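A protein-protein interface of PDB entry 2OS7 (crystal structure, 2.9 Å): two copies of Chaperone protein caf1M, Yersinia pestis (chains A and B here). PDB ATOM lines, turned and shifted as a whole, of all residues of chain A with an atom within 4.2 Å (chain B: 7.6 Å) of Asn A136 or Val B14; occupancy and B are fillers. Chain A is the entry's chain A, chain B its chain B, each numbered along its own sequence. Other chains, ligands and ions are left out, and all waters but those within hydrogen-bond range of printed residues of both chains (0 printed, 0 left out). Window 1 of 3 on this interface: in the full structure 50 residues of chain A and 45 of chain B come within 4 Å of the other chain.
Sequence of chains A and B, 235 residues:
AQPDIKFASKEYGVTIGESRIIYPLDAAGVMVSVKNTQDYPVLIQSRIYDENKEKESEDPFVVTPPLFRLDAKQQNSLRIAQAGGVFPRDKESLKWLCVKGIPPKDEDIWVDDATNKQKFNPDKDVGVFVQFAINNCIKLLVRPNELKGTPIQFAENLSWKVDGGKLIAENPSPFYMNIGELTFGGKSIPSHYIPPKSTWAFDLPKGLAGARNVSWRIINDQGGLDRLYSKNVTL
Among the printed residues, merely in contact across the chains: Val A34 with Val B14 (3.8 Å), Val A34 with Thr B15 (3.4 Å), Lys A35 with Val B14 (3.1 Å), Ile A44 with Val B14 (3.4 Å), Leu A70 with Val B14 (3.9 Å), Val A99 with Val B14 (3.2 Å) and Asn A136 with Ile B16 (3.5 Å).
Of the 6 printed residues of chain B, 4 touch a printed residue of chain A.
Hydrophobic or aromatic side chains of chain B within 4 Å of the printed part of chain A: Val B14 and Ile B16.
Among the printed residues, 10 pairs touch across the chains.
The side-chain sulfur (SG) of Cys A98 is disulfide-bonded to the side-chain sulfur (SG) of Cys A137 (2.1 Å).
The backbone NH of Val A99 is in hydrogen-bond range of the backbone carbonyl oxygen of Asn A136 (2.8 Å).
O of Leu A70 is in hydrogen-bond range of ND2 of Asn A36, at 3.4 Å.
No position is printed for both chains.
Of the printed residues of chain B, Val A99 touches Val B14.
Of the printed residues of chain A, Ile B16 touches Asn A136.
Printed residues of chain B within 4 Å of Val A34: Val B14 (3.8 Å) and Thr B15 (3.4 Å).
Of the printed residues of chain B, Ile A44 touches Val B14 (3.4 Å).
The nearest residue of chain B that does not touch Asn A136 is Thr B15 (4.4 Å).
The nearest residue of chain A that does not touch Val B14 is Asn A36 (4.1 Å).
The backbone carbonyl oxygen (O) of Lys A35 is in hydrogen-bond range of the backbone NH (N) of Thr B15.
The backbone NH of Ile A134 lies within hydrogen-bond range of the backbone carbonyl oxygen of Tyr B12 (2.8 Å).
The backbone carbonyl oxygen of Val B14 is in hydrogen-bond range of the side-chain amide nitrogen of Asn A136 (2.9 Å).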
ATOM      1  N   VAL A  34      21.836 -11.456  10.202  1.00  0.00           N
ATOM      2  CA  VAL A  34      20.647 -10.645   9.916  1.00  0.00           C
ATOM      3  C   VAL A  34      21.102  -9.225   9.741  1.00  0.00           C
ATOM      4  O   VAL A  34      21.924  -8.766  10.526  1.00  0.00           O
ATOM      5  CB  VAL A  34      19.645 -10.731  11.071  1.00  0.00           C
ATOM      6  CG1 VAL A  34      19.375  -9.358  11.699  1.00  0.00           C
ATOM      7  CG2 VAL A  34      18.386 -11.378  10.625  1.00  0.00           C
ATOM      8  N   LYS A  35      20.595  -8.529   8.732  1.00  0.00           N
ATOM      9  CA  LYS A  35      21.202  -7.253   8.342  1.00  0.00           C
ATOM     10  C   LYS A  35      20.238  -6.104   7.998  1.00  0.00           C
ATOM     11  O   LYS A  35      19.295  -6.253   7.232  1.00  0.00           O
ATOM     12  CB  LYS A  35      22.211  -7.445   7.206  1.00  0.00           C
ATOM     13  CG  LYS A  35      23.081  -6.236   7.025  1.00  0.00           C
ATOM     14  CD  LYS A  35      23.914  -6.290   5.793  1.00  0.00           C
ATOM     15  CE  LYS A  35      24.684  -4.986   5.604  1.00  0.00           C
ATOM     16  NZ  LYS A  35      25.802  -4.836   6.613  1.00  0.00           N
ATOM     17  N   ASN A  36      20.513  -4.942   8.559  1.00  0.00           N
ATOM     18  CA  ASN A  36      19.685  -3.805   8.347  1.00  0.00           C
ATOM     19  C   ASN A  36      20.261  -2.944   7.221  1.00  0.00           C
ATOM     20  O   ASN A  36      21.242  -2.221   7.423  1.00  0.00           O
ATOM     21  CB  ASN A  36      19.596  -3.016   9.648  1.00  0.00           C
ATOM     22  CG  ASN A  36      18.928  -1.665   9.482  1.00  0.00           C
ATOM     23  OD1 ASN A  36      18.217  -1.401   8.512  1.00  0.00           O
ATOM     24  ND2 ASN A  36      19.157  -0.794  10.445  1.00  0.00           N
ATOM     25  N   ILE A  44      13.624  -5.373  15.463  1.00  0.00           N
ATOM     26  CA  ILE A  44      13.596  -6.665  14.820  1.00  0.00           C
ATOM     27  C   ILE A  44      12.904  -7.678  15.737  1.00  0.00           C
ATOM     28  O   ILE A  44      13.229  -7.753  16.894  1.00  0.00           O
ATOM     29  CB  ILE A  44      15.087  -7.047  14.364  1.00  0.00           C
ATOM     30  CG1 ILE A  44      15.121  -7.416  12.909  1.00  0.00           C
ATOM     31  CG2 ILE A  44      15.819  -8.131  15.215  1.00  0.00           C
ATOM     32  CD1 ILE A  44      14.644  -6.275  12.063  1.00  0.00           C
ATOM     33  N   LEU A  70      18.339  -2.801  15.941  1.00  0.00           N
ATOM     34  CA  LEU A  70      19.524  -2.904  15.137  1.00  0.00           C
ATOM     35  C   LEU A  70      19.791  -1.546  14.489  1.00  0.00           C
ATOM     36  O   LEU A  70      18.901  -0.982  13.853  1.00  0.00           O
ATOM     37  CB  LEU A  70      19.278  -3.977  14.089  1.00  0.00           C
ATOM     38  CG  LEU A  70      20.395  -4.506  13.213  1.00  0.00           C
ATOM     39  CD1 LEU A  70      21.391  -5.277  14.023  1.00  0.00           C
ATOM     40  CD2 LEU A  70      19.812  -5.411  12.197  1.00  0.00           C
ATOM     41  N   LEU A  97      11.745 -19.544   9.890  1.00  0.00           N
ATOM     42  CA  LEU A  97      12.270 -18.468  10.730  1.00  0.00           C
ATOM     43  C   LEU A  97      11.823 -17.165  10.108  1.00  0.00           C
ATOM     44  O   LEU A  97      12.152 -16.901   8.955  1.00  0.00           O
ATOM     45  CB  LEU A  97      13.805 -18.530  10.788  1.00  0.00           C
ATOM     46  CG  LEU A  97      14.641 -17.264  11.104  1.00  0.00           C
ATOM     47  CD1 LEU A  97      14.640 -16.894  12.544  1.00  0.00           C
ATOM     48  CD2 LEU A  97      16.102 -17.351  10.583  1.00  0.00           C
ATOM     49  N   CYS A  98      11.062 -16.370  10.855  1.00  0.00           N
ATOM     50  CA  CYS A  98      10.520 -15.104  10.344  1.00  0.00           C
ATOM     51  C   CYS A  98      11.092 -13.954  11.120  1.00  0.00           C
ATOM     52  O   CYS A  98      11.166 -13.984  12.339  1.00  0.00           O
ATOM     53  CB  CYS A  98       9.020 -15.078  10.456  1.00  0.00           C
ATOM     54  SG  CYS A  98       8.231 -16.358   9.486  1.00  0.00           S
ATOM     55  N   VAL A  99      11.521 -12.930  10.416  1.00  0.00           N
ATOM     56  CA  VAL A  99      12.069 -11.760  11.066  1.00  0.00           C
ATOM     57  C   VAL A  99      11.381 -10.510  10.551  1.00  0.00           C
ATOM     58  O   VAL A  99      11.562 -10.133   9.396  1.00  0.00           O
ATOM     59  CB  VAL A  99      13.566 -11.657  10.850  1.00  0.00           C
ATOM     60  CG1 VAL A  99      14.063 -10.387  11.491  1.00  0.00           C
ATOM     61  CG2 VAL A  99      14.279 -12.864  11.446  1.00  0.00           C
ATOM     62  N   ILE A 134       8.404  -4.938   6.788  1.00  0.00           N
ATOM     63  CA  ILE A 134       8.715  -6.191   6.050  1.00  0.00           C
ATOM     64  C   ILE A 134       8.774  -7.441   6.938  1.00  0.00           C
ATOM     65  O   ILE A 134       9.606  -7.515   7.848  1.00  0.00           O
ATOM     66  CB  ILE A 134      10.036  -6.089   5.238  1.00  0.00           C
ATOM     67  CG1 ILE A 134       9.994  -4.929   4.231  1.00  0.00           C
ATOM     68  CG2 ILE A 134      10.292  -7.366   4.524  1.00  0.00           C
ATOM     69  CD1 ILE A 134      11.365  -4.287   3.967  1.00  0.00           C
ATOM     70  N   ASN A 135       7.890  -8.405   6.689  1.00  0.00           N
ATOM     71  CA  ASN A 135       7.964  -9.698   7.373  1.00  0.00           C
ATOM     72  C   ASN A 135       8.621 -10.721   6.491  1.00  0.00           C
ATOM     73  O   ASN A 135       8.029 -11.302   5.587  1.00  0.00           O
ATOM     74  CB  ASN A 135       6.616 -10.220   7.859  1.00  0.00           C
ATOM     75  CG  ASN A 135       6.764 -11.459   8.762  1.00  0.00           C
ATOM     76  OD1 ASN A 135       7.554 -11.472   9.713  1.00  0.00           O
ATOM     77  ND2 ASN A 135       5.992 -12.490   8.477  1.00  0.00           N
ATOM     78  N   ASN A 136       9.886 -10.915   6.776  1.00  0.00           N
ATOM     79  CA  ASN A 136      10.740 -11.748   5.968  1.00  0.00           C
ATOM     80  C   ASN A 136      10.890 -13.189   6.547  1.00  0.00           C
ATOM     81  O   ASN A 136      11.443 -13.354   7.615  1.00  0.00           O
ATOM     82  CB  ASN A 136      12.078 -11.044   5.846  1.00  0.00           C
ATOM     83  CG  ASN A 136      13.065 -11.839   5.058  1.00  0.00           C
ATOM     84  OD1 ASN A 136      12.755 -12.950   4.631  1.00  0.00           O
ATOM     85  ND2 ASN A 136      14.281 -11.283   4.848  1.00  0.00           N
ATOM     86  N   CYS A 137      10.360 -14.208   5.869  1.00  0.00           N
ATOM     87  CA  CYS A 137      10.559 -15.583   6.327  1.00  0.00           C
ATOM     88  C   CYS A 137      11.458 -16.379   5.409  1.00  0.00           C
ATOM     89  O   CYS A 137      11.373 -16.234   4.214  1.00  0.00           O
ATOM     90  CB  CYS A 137       9.256 -16.351   6.508  1.00  0.00           C
ATOM     91  SG  CYS A 137       8.085 -15.557   7.588  1.00  0.00           S
ATOM     92  N   TYR B  12      11.065  -0.919   6.844  1.00  0.00           N
ATOM     93  CA  TYR B  12      11.722  -1.600   7.968  1.00  0.00           C
ATOM     94  C   TYR B  12      11.815  -3.113   7.762  1.00  0.00           C
ATOM     95  O   TYR B  12      10.816  -3.781   7.535  1.00  0.00           O
ATOM     96  CB  TYR B  12      10.968  -1.287   9.247  1.00  0.00           C
ATOM     97  CG  TYR B  12      10.829   0.194   9.525  1.00  0.00           C
ATOM     98  CD1 TYR B  12       9.712   0.891   9.079  1.00  0.00           C
ATOM     99  CD2 TYR B  12      11.801   0.898  10.252  1.00  0.00           C
ATOM    100  CE1 TYR B  12       9.564   2.269   9.334  1.00  0.00           C
ATOM    101  CE2 TYR B  12      11.655   2.255  10.518  1.00  0.00           C
ATOM    102  CZ  TYR B  12      10.531   2.939  10.050  1.00  0.00           C
ATOM    103  OH  TYR B  12      10.349   4.287  10.280  1.00  0.00           O
ATOM    104  N   GLY B  13      13.016  -3.654   7.820  1.00  0.00           N
ATOM    105  CA  GLY B  13      13.209  -5.081   7.570  1.00  0.00           C
ATOM    106  C   GLY B  13      14.661  -5.474   7.490  1.00  0.00           C
ATOM    107  O   GLY B  13      15.547  -4.628   7.463  1.00  0.00           O
ATOM    108  N   VAL B  14      14.919  -6.767   7.458  1.00  0.00           N
ATOM    109  CA  VAL B  14      16.306  -7.219   7.396  1.00  0.00           C
ATOM    110  C   VAL B  14      16.538  -8.193   6.277  1.00  0.00           C
ATOM    111  O   VAL B  14      15.616  -8.852   5.804  1.00  0.00           O
ATOM    112  CB  VAL B  14      16.796  -7.850   8.731  1.00  0.00           C
ATOM    113  CG1 VAL B  14      17.049  -6.796   9.784  1.00  0.00           C
ATOM    114  CG2 VAL B  14      15.840  -8.876   9.230  1.00  0.00           C
ATOM    115  N   THR B  15      17.783  -8.273   5.858  1.00  0.00           N
ATOM    116  CA  THR B  15      18.250  -9.340   4.997  1.00  0.00           C
ATOM    117  C   THR B  15      18.585 -10.543   5.880  1.00  0.00           C
ATOM    118  O   THR B  15      19.305 -10.418   6.847  1.00  0.00           O
ATOM    119  CB  THR B  15      19.510  -8.860   4.209  1.00  0.00           C
ATOM    120  OG1 THR B  15      19.091  -8.239   2.997  1.00  0.00           O
ATOM    121  CG2 THR B  15      20.500 -10.005   3.869  1.00  0.00           C
ATOM    122  N   ILE B  16      18.045 -11.708   5.569  1.00  0.00           N
ATOM    123  CA  ILE B  16      18.464 -12.899   6.291  1.00  0.00           C
ATOM    124  C   ILE B  16      19.545 -13.636   5.500  1.00  0.00           C
ATOM    125  O   ILE B  16      19.324 -14.053   4.360  1.00  0.00           O
ATOM    126  CB  ILE B  16      17.300 -13.817   6.503  1.00  0.00           C
ATOM    127  CG1 ILE B  16      16.257 -13.086   7.326  1.00  0.00           C
ATOM    128  CG2 ILE B  16      17.736 -15.023   7.228  1.00  0.00           C
ATOM    129  CD1 ILE B  16      14.874 -13.753   7.353  1.00  0.00           C
ATOM    130  N   GLY B  17      20.714 -13.809   6.087  1.00  0.00           N
ATOM    131  CA  GLY B  17      21.717 -14.655   5.440  1.00  0.00           C
ATOM    132  C   GLY B  17      22.325 -14.112   4.158  1.00  0.00           C
ATOM    133  O   GLY B  17      22.350 -12.892   3.935  1.00  0.00           O
